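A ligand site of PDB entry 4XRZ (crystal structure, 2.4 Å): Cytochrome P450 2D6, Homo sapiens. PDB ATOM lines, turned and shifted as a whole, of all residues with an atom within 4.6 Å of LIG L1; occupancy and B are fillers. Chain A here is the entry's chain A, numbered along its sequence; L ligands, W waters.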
ATOM      1  N   ARG A  79      37.675  11.384 -18.995  1.00  0.00           N
ATOM      2  CA  ARG A  79      37.522  12.817 -18.772  1.00  0.00           C
ATOM      3  C   ARG A  79      38.329  13.620 -19.784  1.00  0.00           C
ATOM      4  O   ARG A  79      39.406  13.181 -20.198  1.00  0.00           O
ATOM      5  CB  ARG A  79      37.946  13.190 -17.351  1.00  0.00           C
ATOM      6  CG  ARG A  79      37.143  12.554 -16.242  1.00  0.00           C
ATOM      7  CD  ARG A  79      35.759  13.173 -16.111  1.00  0.00           C
ATOM      8  NE  ARG A  79      35.085  12.742 -14.899  1.00  0.00           N
ATOM      9  CZ  ARG A  79      33.772  12.579 -14.787  1.00  0.00           C
ATOM     10  NH1 ARG A  79      33.246  12.182 -13.630  1.00  0.00           N
ATOM     11  NH2 ARG A  79      32.978  12.812 -15.819  1.00  0.00           N
ATOM     12  N   VAL A  97      39.687  11.625  -8.143  1.00  0.00           N
ATOM     13  CA  VAL A  97      38.662  10.811  -8.776  1.00  0.00           C
ATOM     14  C   VAL A  97      37.912  11.599  -9.843  1.00  0.00           C
ATOM     15  O   VAL A  97      37.732  11.130 -10.969  1.00  0.00           O
ATOM     16  CB  VAL A  97      37.639  10.282  -7.742  1.00  0.00           C
ATOM     17  CG1 VAL A  97      36.466   9.615  -8.447  1.00  0.00           C
ATOM     18  CG2 VAL A  97      38.306   9.319  -6.782  1.00  0.00           C
ATOM     19  N   PHE A  98      37.486  12.804  -9.478  1.00  0.00           N
ATOM     20  CA  PHE A  98      36.585  13.616 -10.289  1.00  0.00           C
ATOM     21  C   PHE A  98      37.092  13.893 -11.704  1.00  0.00           C
ATOM     22  O   PHE A  98      36.397  13.602 -12.675  1.00  0.00           O
ATOM     23  CB  PHE A  98      36.310  14.939  -9.588  1.00  0.00           C
ATOM     24  CG  PHE A  98      34.848  15.193  -9.350  1.00  0.00           C
ATOM     25  CD1 PHE A  98      34.287  14.909  -8.123  1.00  0.00           C
ATOM     26  CD2 PHE A  98      34.052  15.710 -10.357  1.00  0.00           C
ATOM     27  CE1 PHE A  98      32.943  15.144  -7.901  1.00  0.00           C
ATOM     28  CE2 PHE A  98      32.709  15.939 -10.142  1.00  0.00           C
ATOM     29  CZ  PHE A  98      32.155  15.650  -8.910  1.00  0.00           C
ATOM     30  N   TRP A 106      42.417   6.413 -11.459  1.00  0.00           N
ATOM     31  CA  TRP A 106      41.019   6.699 -11.171  1.00  0.00           C
ATOM     32  C   TRP A 106      40.355   5.527 -10.456  1.00  0.00           C
ATOM     33  O   TRP A 106      39.627   5.704  -9.486  1.00  0.00           O
ATOM     34  CB  TRP A 106      40.245   7.024 -12.459  1.00  0.00           C
ATOM     35  CG  TRP A 106      38.757   6.905 -12.284  1.00  0.00           C
ATOM     36  CD1 TRP A 106      37.927   7.846 -11.771  1.00  0.00           C
ATOM     37  CD2 TRP A 106      37.938   5.773 -12.616  1.00  0.00           C
ATOM     38  NE1 TRP A 106      36.624   7.377 -11.756  1.00  0.00           N
ATOM     39  CE2 TRP A 106      36.616   6.110 -12.278  1.00  0.00           C
ATOM     40  CE3 TRP A 106      38.202   4.515 -13.163  1.00  0.00           C
ATOM     41  CZ2 TRP A 106      35.550   5.235 -12.475  1.00  0.00           C
ATOM     42  CZ3 TRP A 106      37.150   3.642 -13.359  1.00  0.00           C
ATOM     43  CH2 TRP A 106      35.837   4.011 -13.006  1.00  0.00           C
ATOM     44  N   ARG A 110      38.744   5.448  -6.762  1.00  0.00           N
ATOM     45  CA  ARG A 110      37.294   5.284  -6.765  1.00  0.00           C
ATOM     46  C   ARG A 110      36.870   4.090  -5.911  1.00  0.00           C
ATOM     47  O   ARG A 110      35.980   4.202  -5.072  1.00  0.00           O
ATOM     48  CB  ARG A 110      36.767   5.117  -8.192  1.00  0.00           C
ATOM     49  CG  ARG A 110      35.374   4.510  -8.262  1.00  0.00           C
ATOM     50  CD  ARG A 110      34.402   5.391  -9.025  1.00  0.00           C
ATOM     51  NE  ARG A 110      33.036   4.912  -8.882  1.00  0.00           N
ATOM     52  CZ  ARG A 110      31.958   5.610  -9.235  1.00  0.00           C
ATOM     53  NH1 ARG A 110      32.098   6.820  -9.759  1.00  0.00           N
ATOM     54  NH2 ARG A 110      30.747   5.097  -9.076  1.00  0.00           N
ATOM     55  N   ILE A 164      30.190  14.905   6.195  1.00  0.00           N
ATOM     56  CA  ILE A 164      31.280  14.476   5.341  1.00  0.00           C
ATOM     57  C   ILE A 164      32.636  14.710   6.018  1.00  0.00           C
ATOM     58  O   ILE A 164      33.580  13.948   5.810  1.00  0.00           O
ATOM     59  CB  ILE A 164      31.246  15.184   3.957  1.00  0.00           C
ATOM     60  CG1 ILE A 164      32.313  14.604   3.027  1.00  0.00           C
ATOM     61  CG2 ILE A 164      31.409  16.687   4.100  1.00  0.00           C
ATOM     62  CD1 ILE A 164      32.204  13.108   2.809  1.00  0.00           C
ATOM     63  N   LEU A 280      35.996  15.283  -1.994  1.00  0.00           N
ATOM     64  CA  LEU A 280      34.962  14.658  -1.171  1.00  0.00           C
ATOM     65  C   LEU A 280      34.262  15.650  -0.244  1.00  0.00           C
ATOM     66  O   LEU A 280      33.028  15.692  -0.197  1.00  0.00           O
ATOM     67  CB  LEU A 280      35.576  13.523  -0.339  1.00  0.00           C
ATOM     68  CG  LEU A 280      35.893  12.215  -1.072  1.00  0.00           C
ATOM     69  CD1 LEU A 280      36.467  11.199  -0.096  1.00  0.00           C
ATOM     70  CD2 LEU A 280      34.642  11.674  -1.750  1.00  0.00           C
ATOM     71  N   ALA A 283      32.288  18.316  -2.240  1.00  0.00           N
ATOM     72  CA  ALA A 283      31.148  17.634  -2.846  1.00  0.00           C
ATOM     73  C   ALA A 283      30.112  17.322  -1.785  1.00  0.00           C
ATOM     74  O   ALA A 283      28.913  17.541  -1.984  1.00  0.00           O
ATOM     75  CB  ALA A 283      31.580  16.358  -3.545  1.00  0.00           C
ATOM     76  N   GLY A 284      30.587  16.804  -0.651  1.00  0.00           N
ATOM     77  CA  GLY A 284      29.735  16.490   0.470  1.00  0.00           C
ATOM     78  C   GLY A 284      28.952  17.699   0.940  1.00  0.00           C
ATOM     79  O   GLY A 284      27.850  17.574   1.452  1.00  0.00           O
ATOM     80  N   THR A 287      26.489  19.876  -2.680  1.00  0.00           N
ATOM     81  CA  THR A 287      25.466  19.119  -3.388  1.00  0.00           C
ATOM     82  C   THR A 287      24.235  18.879  -2.513  1.00  0.00           C
ATOM     83  O   THR A 287      23.129  19.291  -2.869  1.00  0.00           O
ATOM     84  CB  THR A 287      26.001  17.750  -3.860  1.00  0.00           C
ATOM     85  OG1 THR A 287      26.469  17.002  -2.732  1.00  0.00           O
ATOM     86  CG2 THR A 287      27.132  17.940  -4.868  1.00  0.00           C
ATOM     87  N   THR A 288      24.437  18.226  -1.381  1.00  0.00           N
ATOM     88  CA  THR A 288      23.342  17.843  -0.495  1.00  0.00           C
ATOM     89  C   THR A 288      22.643  19.066   0.122  1.00  0.00           C
ATOM     90  O   THR A 288      21.431  19.064   0.302  1.00  0.00           O
ATOM     91  CB  THR A 288      23.846  16.911   0.621  1.00  0.00           C
ATOM     92  OG1 THR A 288      24.393  15.733   0.032  1.00  0.00           O
ATOM     93  CG2 THR A 288      22.715  16.515   1.552  1.00  0.00           C
ATOM     94  N   THR A 291      20.510  20.876  -2.516  1.00  0.00           N
ATOM     95  CA  THR A 291      19.319  20.065  -2.709  1.00  0.00           C
ATOM     96  C   THR A 291      18.331  20.301  -1.570  1.00  0.00           C
ATOM     97  O   THR A 291      17.128  20.418  -1.789  1.00  0.00           O
ATOM     98  CB  THR A 291      19.663  18.561  -2.800  1.00  0.00           C
ATOM     99  OG1 THR A 291      20.635  18.350  -3.830  1.00  0.00           O
ATOM    100  CG2 THR A 291      18.413  17.755  -3.099  1.00  0.00           C
ATOM    101  N   GLN A 342      14.924  16.550  -5.988  1.00  0.00           N
ATOM    102  CA  GLN A 342      16.109  16.321  -6.795  1.00  0.00           C
ATOM    103  C   GLN A 342      15.834  16.539  -8.274  1.00  0.00           C
ATOM    104  O   GLN A 342      16.615  17.179  -8.983  1.00  0.00           O
ATOM    105  CB  GLN A 342      16.660  14.911  -6.573  1.00  0.00           C
ATOM    106  CG  GLN A 342      17.189  14.654  -5.173  1.00  0.00           C
ATOM    107  CD  GLN A 342      18.187  13.510  -5.146  1.00  0.00           C
ATOM    108  OE1 GLN A 342      17.836  12.357  -4.878  1.00  0.00           O
ATOM    109  NE2 GLN A 342      19.456  13.828  -5.422  1.00  0.00           N
ATOM    110  N   ILE A 347      20.191  20.126  -9.791  1.00  0.00           N
ATOM    111  CA  ILE A 347      21.331  20.901  -9.328  1.00  0.00           C
ATOM    112  C   ILE A 347      22.604  20.717 -10.170  1.00  0.00           C
ATOM    113  O   ILE A 347      23.513  21.539 -10.102  1.00  0.00           O
ATOM    114  CB  ILE A 347      21.667  20.568  -7.860  1.00  0.00           C
ATOM    115  CG1 ILE A 347      22.271  19.170  -7.731  1.00  0.00           C
ATOM    116  CG2 ILE A 347      20.423  20.695  -6.992  1.00  0.00           C
ATOM    117  CD1 ILE A 347      22.820  18.878  -6.352  1.00  0.00           C
ATOM    118  N   VAL A 348      22.664  19.652 -10.966  1.00  0.00           N
ATOM    119  CA  VAL A 348      23.784  19.473 -11.892  1.00  0.00           C
ATOM    120  C   VAL A 348      23.233  19.275 -13.309  1.00  0.00           C
ATOM    121  O   VAL A 348      23.230  18.161 -13.827  1.00  0.00           O
ATOM    122  CB  VAL A 348      24.675  18.268 -11.530  1.00  0.00           C
ATOM    123  CG1 VAL A 348      26.076  18.468 -12.091  1.00  0.00           C
ATOM    124  CG2 VAL A 348      24.763  18.100 -10.022  1.00  0.00           C
ATOM    125  N   GLY A 351      25.691  18.000 -15.869  1.00  0.00           N
ATOM    126  CA  GLY A 351      26.520  16.948 -15.318  1.00  0.00           C
ATOM    127  C   GLY A 351      27.997  17.307 -15.289  1.00  0.00           C
ATOM    128  O   GLY A 351      28.360  18.477 -15.135  1.00  0.00           O
ATOM    129  N   VAL A 352      28.841  16.295 -15.438  1.00  0.00           N
ATOM    130  CA  VAL A 352      30.275  16.509 -15.571  1.00  0.00           C
ATOM    131  C   VAL A 352      30.723  15.997 -16.930  1.00  0.00           C
ATOM    132  O   VAL A 352      30.293  14.926 -17.363  1.00  0.00           O
ATOM    133  CB  VAL A 352      31.052  15.802 -14.436  1.00  0.00           C
ATOM    134  CG1 VAL A 352      32.550  15.955 -14.639  1.00  0.00           C
ATOM    135  CG2 VAL A 352      30.629  16.346 -13.086  1.00  0.00           C
ATOM    136  N   HIS A 354      32.355  14.312 -20.058  1.00  0.00           N
ATOM    137  CA  HIS A 354      33.068  13.090 -20.371  1.00  0.00           C
ATOM    138  C   HIS A 354      33.895  13.287 -21.636  1.00  0.00           C
ATOM    139  O   HIS A 354      33.808  14.336 -22.276  1.00  0.00           O
ATOM    140  CB  HIS A 354      32.097  11.919 -20.566  1.00  0.00           C
ATOM    141  CG  HIS A 354      31.376  11.506 -19.326  1.00  0.00           C
ATOM    142  ND1 HIS A 354      31.475  10.232 -18.798  1.00  0.00           N
ATOM    143  CD2 HIS A 354      30.543  12.188 -18.505  1.00  0.00           C
ATOM    144  CE1 HIS A 354      30.738  10.156 -17.709  1.00  0.00           C
ATOM    145  NE2 HIS A 354      30.161  11.324 -17.511  1.00  0.00           N
ATOM    146  N   LEU A 377      21.775  16.307 -18.322  1.00  0.00           N
ATOM    147  CA  LEU A 377      20.954  15.604 -17.344  1.00  0.00           C
ATOM    148  C   LEU A 377      19.640  16.334 -17.082  1.00  0.00           C
ATOM    149  O   LEU A 377      18.641  15.719 -16.709  1.00  0.00           O
ATOM    150  CB  LEU A 377      21.727  15.422 -16.030  1.00  0.00           C
ATOM    151  CG  LEU A 377      23.051  14.668 -16.125  1.00  0.00           C
ATOM    152  CD1 LEU A 377      23.725  14.603 -14.781  1.00  0.00           C
ATOM    153  CD2 LEU A 377      22.814  13.271 -16.671  1.00  0.00           C
ATOM    154  N   PRO A 413      19.747  11.959 -11.564  1.00  0.00           N
ATOM    155  CA  PRO A 413      20.442  13.151 -11.067  1.00  0.00           C
ATOM    156  C   PRO A 413      21.913  12.885 -10.741  1.00  0.00           C
ATOM    157  O   PRO A 413      22.703  13.815 -10.640  1.00  0.00           O
ATOM    158  CB  PRO A 413      19.663  13.522  -9.808  1.00  0.00           C
ATOM    159  CG  PRO A 413      19.152  12.213  -9.307  1.00  0.00           C
ATOM    160  CD  PRO A 413      18.862  11.375 -10.525  1.00  0.00           C
ATOM    161  N   PHE A 414      22.260  11.614 -10.592  1.00  0.00           N
ATOM    162  CA  PHE A 414      23.633  11.211 -10.315  1.00  0.00           C
ATOM    163  C   PHE A 414      24.309  10.666 -11.567  1.00  0.00           C
ATOM    164  O   PHE A 414      25.304   9.945 -11.471  1.00  0.00           O
ATOM    165  CB  PHE A 414      23.675  10.164  -9.197  1.00  0.00           C
ATOM    166  CG  PHE A 414      23.008  10.600  -7.932  1.00  0.00           C
ATOM    167  CD1 PHE A 414      21.717  10.192  -7.639  1.00  0.00           C
ATOM    168  CD2 PHE A 414      23.661  11.418  -7.026  1.00  0.00           C
ATOM    169  CE1 PHE A 414      21.088  10.591  -6.466  1.00  0.00           C
ATOM    170  CE2 PHE A 414      23.046  11.818  -5.853  1.00  0.00           C
ATOM    171  CZ  PHE A 414      21.763  11.411  -5.572  1.00  0.00           C
ATOM    172  N   SER A 415      23.751  10.989 -12.723  1.00  0.00           N
ATOM    173  CA  SER A 415      24.220  10.497 -14.016  1.00  0.00           C
ATOM    174  C   SER A 415      24.165   8.966 -14.064  1.00  0.00           C
ATOM    175  O   SER A 415      23.402   8.338 -13.335  1.00  0.00           O
ATOM    176  CB  SER A 415      25.635  10.987 -14.305  1.00  0.00           C
ATOM    177  OG  SER A 415      26.052  10.605 -15.606  1.00  0.00           O
ATOM    178  N   ALA A 416      24.981   8.366 -14.930  1.00  0.00           N
ATOM    179  CA  ALA A 416      24.962   6.917 -15.105  1.00  0.00           C
ATOM    180  C   ALA A 416      26.294   6.394 -15.641  1.00  0.00           C
ATOM    181  O   ALA A 416      27.131   7.162 -16.119  1.00  0.00           O
ATOM    182  CB  ALA A 416      23.833   6.506 -16.041  1.00  0.00           C
ATOM    183  N   ARG A 418      30.016   4.085 -15.458  1.00  0.00           N
ATOM    184  CA  ARG A 418      31.148   3.884 -14.551  1.00  0.00           C
ATOM    185  C   ARG A 418      31.526   5.116 -13.736  1.00  0.00           C
ATOM    186  O   ARG A 418      32.164   5.013 -12.695  1.00  0.00           O
ATOM    187  CB  ARG A 418      32.377   3.417 -15.348  1.00  0.00           C
ATOM    188  CG  ARG A 418      32.249   2.006 -15.890  1.00  0.00           C
ATOM    189  CD  ARG A 418      33.366   1.669 -16.869  1.00  0.00           C
ATOM    190  NE  ARG A 418      33.352   0.261 -17.260  1.00  0.00           N
ATOM    191  CZ  ARG A 418      32.573  -0.240 -18.204  1.00  0.00           C
ATOM    192  NH1 ARG A 418      32.623  -1.536 -18.494  1.00  0.00           N
ATOM    193  NH2 ARG A 418      31.734   0.541 -18.873  1.00  0.00           N
ATOM    194  N   ARG A 419      31.125   6.291 -14.209  1.00  0.00           N
ATOM    195  CA  ARG A 419      31.486   7.548 -13.549  1.00  0.00           C
ATOM    196  C   ARG A 419      30.366   8.120 -12.688  1.00  0.00           C
ATOM    197  O   ARG A 419      30.539   9.174 -12.078  1.00  0.00           O
ATOM    198  CB  ARG A 419      31.893   8.587 -14.593  1.00  0.00           C
ATOM    199  CG  ARG A 419      33.238   8.338 -15.236  1.00  0.00           C
ATOM    200  CD  ARG A 419      34.361   8.393 -14.215  1.00  0.00           C
ATOM    201  NE  ARG A 419      35.665   8.502 -14.849  1.00  0.00           N
ATOM    202  CZ  ARG A 419      36.569   9.421 -14.547  1.00  0.00           C
ATOM    203  NH1 ARG A 419      36.341  10.316 -13.599  1.00  0.00           N
ATOM    204  NH2 ARG A 419      37.731   9.431 -15.190  1.00  0.00           N
ATOM    205  N   ALA A 420      29.240   7.412 -12.627  1.00  0.00           N
ATOM    206  CA  ALA A 420      28.086   7.861 -11.840  1.00  0.00           C
ATOM    207  C   ALA A 420      28.496   8.180 -10.404  1.00  0.00           C
ATOM    208  O   ALA A 420      29.353   7.504  -9.833  1.00  0.00           O
ATOM    209  CB  ALA A 420      26.987   6.816 -11.849  1.00  0.00           C
ATOM    210  N   CYS A 421      27.886   9.218  -9.841  1.00  0.00           N
ATOM    211  CA  CYS A 421      28.240   9.747  -8.524  1.00  0.00           C
ATOM    212  C   CYS A 421      28.443   8.653  -7.471  1.00  0.00           C
ATOM    213  O   CYS A 421      27.542   7.857  -7.204  1.00  0.00           O
ATOM    214  CB  CYS A 421      27.171  10.725  -8.058  1.00  0.00           C
ATOM    215  SG  CYS A 421      27.504  11.483  -6.449  1.00  0.00           S
ATOM    216  N   LEU A 422      29.639   8.609  -6.893  1.00  0.00           N
ATOM    217  CA  LEU A 422      29.943   7.610  -5.874  1.00  0.00           C
ATOM    218  C   LEU A 422      29.382   8.028  -4.522  1.00  0.00           C
ATOM    219  O   LEU A 422      29.337   7.227  -3.586  1.00  0.00           O
ATOM    220  CB  LEU A 422      31.465   7.366  -5.768  1.00  0.00           C
ATOM    221  CG  LEU A 422      32.467   8.459  -5.384  1.00  0.00           C
ATOM    222  CD1 LEU A 422      32.501   8.729  -3.881  1.00  0.00           C
ATOM    223  CD2 LEU A 422      33.851   8.094  -5.884  1.00  0.00           C
ATOM    224  N   GLY A 423      28.948   9.278  -4.433  1.00  0.00           N
ATOM    225  CA  GLY A 423      28.397   9.811  -3.201  1.00  0.00           C
ATOM    226  C   GLY A 423      26.903   9.605  -3.072  1.00  0.00           C
ATOM    227  O   GLY A 423      26.296  10.019  -2.080  1.00  0.00           O
ATOM    228  N   LEU A 426      25.544   8.144   0.150  1.00  0.00           N
ATOM    229  CA  LEU A 426      25.619   9.120   1.229  1.00  0.00           C
ATOM    230  C   LEU A 426      24.560  10.194   1.052  1.00  0.00           C
ATOM    231  O   LEU A 426      23.928  10.632   2.020  1.00  0.00           O
ATOM    232  CB  LEU A 426      27.014   9.757   1.301  1.00  0.00           C
ATOM    233  CG  LEU A 426      27.172  10.795   2.409  1.00  0.00           C
ATOM    234  CD1 LEU A 426      26.972  10.167   3.777  1.00  0.00           C
ATOM    235  CD2 LEU A 426      28.538  11.484   2.327  1.00  0.00           C
ATOM    236  N   ALA A 427      24.355  10.619  -0.193  1.00  0.00           N
ATOM    237  CA  ALA A 427      23.362  11.632  -0.505  1.00  0.00           C
ATOM    238  C   ALA A 427      21.963  11.156  -0.147  1.00  0.00           C
ATOM    239  O   ALA A 427      21.196  11.884   0.490  1.00  0.00           O
ATOM    240  CB  ALA A 427      23.435  12.002  -1.983  1.00  0.00           C
ATOM    241  N   LEU A 431      19.831  13.085   2.623  1.00  0.00           N
ATOM    242  CA  LEU A 431      18.629  13.779   2.172  1.00  0.00           C
ATOM    243  C   LEU A 431      17.405  13.332   2.957  1.00  0.00           C
ATOM    244  O   LEU A 431      16.594  14.149   3.354  1.00  0.00           O
ATOM    245  CB  LEU A 431      18.408  13.558   0.674  1.00  0.00           C
ATOM    246  CG  LEU A 431      19.354  14.318  -0.264  1.00  0.00           C
ATOM    247  CD1 LEU A 431      18.993  14.063  -1.719  1.00  0.00           C
ATOM    248  CD2 LEU A 431      19.353  15.796   0.068  1.00  0.00           C
HETATM  249  C1  LIG L   1      30.110  12.635  -9.704  1.00  0.00           C
HETATM  250  C2  LIG L   1      25.658  14.369  -8.815  1.00  0.00           C
HETATM  251  C3  LIG L   1      26.537  14.109  -4.053  1.00  0.00           C
HETATM  252  C4  LIG L   1      31.106  12.778  -4.955  1.00  0.00           C
HETATM  253  C5  LIG L   1      28.837  13.148  -9.898  1.00  0.00           C
HETATM  254  C6  LIG L   1      28.213  13.462 -11.165  1.00  0.00           C
HETATM  255  C7  LIG L   1      26.988  13.940 -10.914  1.00  0.00           C
HETATM  256  C8  LIG L   1      26.788  13.945  -9.482  1.00  0.00           C
HETATM  257  C9  LIG L   1      25.997  14.388 -11.964  1.00  0.00           C
HETATM  258  C10 LIG L   1      28.855  13.280 -12.555  1.00  0.00           C
HETATM  259  C11 LIG L   1      28.879  11.820 -12.989  1.00  0.00           C
HETATM  260  C12 LIG L   1      29.480  11.716 -14.372  1.00  0.00           C
HETATM  261  O1  LIG L   1      30.676  12.045 -14.525  1.00  0.00           O
HETATM  262  O2  LIG L   1      28.764  11.318 -15.323  1.00  0.00           O
HETATM  263  C13 LIG L   1      25.484  14.449  -7.441  1.00  0.00           C
HETATM  264  C14 LIG L   1      24.294  14.879  -6.737  1.00  0.00           C
HETATM  265  C15 LIG L   1      24.547  14.814  -5.415  1.00  0.00           C
HETATM  266  C16 LIG L   1      25.896  14.327  -5.256  1.00  0.00           C
HETATM  267  C17 LIG L   1      23.028  15.330  -7.443  1.00  0.00           C
HETATM  268  C18 LIG L   1      23.640  15.145  -4.198  1.00  0.00           C
HETATM  269  C19 LIG L   1      22.372  15.542  -4.255  1.00  0.00           C
HETATM  270  C20 LIG L   1      27.836  13.705  -3.866  1.00  0.00           C
HETATM  271  C21 LIG L   1      28.487  13.442  -2.598  1.00  0.00           C
HETATM  272  C22 LIG L   1      29.759  13.077  -2.843  1.00  0.00           C
HETATM  273  C23 LIG L   1      29.942  13.098  -4.286  1.00  0.00           C
HETATM  274  C24 LIG L   1      27.791  13.581  -1.262  1.00  0.00           C
HETATM  275  C25 LIG L   1      30.889  12.678  -1.862  1.00  0.00           C
HETATM  276  C26 LIG L   1      30.773  12.593  -0.537  1.00  0.00           C
HETATM  277  C27 LIG L   1      31.224  12.591  -6.316  1.00  0.00           C
HETATM  278  C28 LIG L   1      32.402  12.090  -7.003  1.00  0.00           C
HETATM  279  C29 LIG L   1      32.122  12.054  -8.310  1.00  0.00           C
HETATM  280  C30 LIG L   1      30.769  12.526  -8.497  1.00  0.00           C
HETATM  281  C31 LIG L   1      33.706  11.698  -6.365  1.00  0.00           C
HETATM  282  C32 LIG L   1      33.080  11.592  -9.436  1.00  0.00           C
HETATM  283  C33 LIG L   1      32.907  10.092  -9.662  1.00  0.00           C
HETATM  284  C34 LIG L   1      33.811   9.651 -10.789  1.00  0.00           C
HETATM  285  O3  LIG L   1      34.037   8.422 -10.946  1.00  0.00           O
HETATM  286  O4  LIG L   1      34.321  10.529 -11.522  1.00  0.00           O
HETATM  287  N1  LIG L   1      27.937  13.455  -8.895  1.00  0.00           N
HETATM  288  N2  LIG L   1      26.442  14.114  -6.505  1.00  0.00           N
HETATM  289  N3  LIG L   1      28.758  13.483  -4.871  1.00  0.00           N
HETATM  290  N4  LIG L   1      30.251  12.841  -7.262  1.00  0.00           N
HETATM  291 FE1  LIG L   1      28.336  13.530  -6.903  1.00  0.00          FE
HETATM  292  C1  LG2 L   2      35.395  23.407  -6.783  1.00  0.00           C
HETATM  293  C2  LG2 L   2      34.669  22.328  -7.275  1.00  0.00           C
HETATM  294  C3  LG2 L   2      33.620  21.743  -6.554  1.00  0.00           C
HETATM  295  C4  LG2 L   2      33.318  22.327  -5.294  1.00  0.00           C
HETATM  296  C5  LG2 L   2      34.027  23.413  -4.772  1.00  0.00           C
HETATM  297  C6  LG2 L   2      35.066  23.933  -5.533  1.00  0.00           C
HETATM  298  F1  LG2 L   2      35.782  24.940  -5.049  1.00  0.00           F
HETATM  299  F2  LG2 L   2      32.324  21.879  -4.519  1.00  0.00           F
HETATM  300  C7  LG2 L   2      32.905  20.520  -7.107  1.00  0.00           C
HETATM  301  C8  LG2 L   2      31.409  20.806  -7.296  1.00  0.00           C
HETATM  302  O1  LG2 L   2      30.677  19.628  -7.640  1.00  0.00           O
HETATM  303  C9  LG2 L   2      30.778  18.603  -6.636  1.00  0.00           C
HETATM  304  C10 LG2 L   2      32.219  18.137  -6.518  1.00  0.00           C
HETATM  305  C11 LG2 L   2      33.090  19.335  -6.125  1.00  0.00           C
HETATM  306  C12 LG2 L   2      34.569  18.946  -5.998  1.00  0.00           C
HETATM  307  S1  LG2 L   2      35.363  18.474  -7.552  1.00  0.00           S
HETATM  308  C13 LG2 L   2      34.386  19.425  -8.716  1.00  0.00           C
HETATM  309  N1  LG2 L   2      33.397  20.236  -8.477  1.00  0.00           N
HETATM  310  N2  LG2 L   2      34.795  19.229 -10.004  1.00  0.00           N
HETATM  311  C14 LG2 L   2      29.898  17.495  -7.118  1.00  0.00           C
HETATM  312  C15 LG2 L   2      29.022  17.531  -8.197  1.00  0.00           C
HETATM  313  N3  LG2 L   2      28.437  16.279  -8.243  1.00  0.00           N
HETATM  314  N4  LG2 L   2      28.874  15.448  -7.263  1.00  0.00           N
HETATM  315  C16 LG2 L   2      29.779  16.180  -6.556  1.00  0.00           C
HETATM  316  O   HOH W   1      27.429  13.819 -16.109  1.00  0.00           O
HETATM  317  O   HOH W   2      19.824  16.602  -6.013  1.00  0.00           O
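SG of Cys 421 is bound to FE1 of LIG L1 (2.3 Å).
NE2 of His 354 is in hydrogen-bond range of O2 of LIG L1, 2.6 Å away.
An oxygen (O1) of LIG L1 lies within salt-bridge range of the guanidinium group (NH1) of Arg 79.
The guanidinium group (NH1) of Arg 110 is in salt-bridge range of an oxygen (O3) of LIG L1, 2.8 Å away.
O2 of LIG L1 lies within hydrogen-bond range of OG of Ser 415 (2.8 Å).
The indole nitrogen of Trp 106 lies within hydrogen-bond range of an oxygen (O3) of LIG L1 (2.9 Å).
An oxygen (O4) of LIG L1 lies within salt-bridge range of the guanidinium group (NH1) of Arg 419 (2.9 Å).
A nitrogen (N4) of LG2 L2 is bound to an iron atom (FE1) of LIG L1, 2.0 Å away.
The backbone carbonyl oxygen (O) of Phe 414 sits at hydrogen-bond distance from the backbone NH (N) of Cys 421 (3.1 Å).
SG of Cys 421 lies close to N of Gly 423 (3.3 Å).
The guanidinium group (NE) of Arg 79 sits at hydrogen-bond distance from the backbone carbonyl oxygen (O) of Phe 98 (2.7 Å).
NH1 of Arg 110 is in hydrogen-bond range of O of Ala 420 (2.8 Å).
NH1 of Arg 110 lies within hydrogen-bond range of O of Arg 418 (3.4 Å).
The backbone carbonyl oxygen of Phe 98 is in hydrogen-bond range of the guanidinium group of Arg 419, 3.4 Å away.
The guanidinium group of Arg 419 sits at hydrogen-bond distance from the backbone carbonyl oxygen of Val 97 (3.1 Å).
OG1 of Thr 291 is in hydrogen-bond range of O of Thr 287 (2.8 Å).
Val 97 touches LIG L1 (O to O4, 3.5 Å).
CE1 of Phe 98 touches C29 of LIG L1, 3.2 Å away.
CD1 of Ile 164 touches C26 of LIG L1 (3.7 Å).
O of Leu 280 touches C26 of LIG L1, 3.8 Å away.
Ala 283 touches LIG L1 (CB to C23, 3.7 Å).
CA of Gly 284 touches C24 of LIG L1 (3.9 Å).
OG1 of Thr 287 touches C3 of LIG L1, 3.2 Å away.
Thr 291 touches LIG L1.
Gln 342 touches LIG L1 (NE2 to C19, 3.6 Å).
CD1 of Ile 347 touches C17 of LIG L1, at 3.7 Å.
Val 352 touches LIG L1 (CG2 to C10, 3.6 Å).
Leu 377 touches LIG L1 (CD1 to C9, 3.6 Å).
Pro 413 touches LIG L1 (O to C2, 3.5 Å).
Phe 414 touches LIG L1.
Leu 422 touches LIG L1.
Gly 423 touches LIG L1.
Leu 426 touches LIG L1.
CB of Ala 427 touches C18 of LIG L1 (3.9 Å).
Water W1 bridges the backbone NH (N) of Val 352 and an oxygen (O2) of LIG L1.
Water W2 bridges the side-chain amide nitrogen of Gln 342 and the side-chain hydroxyl of Thr 291.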
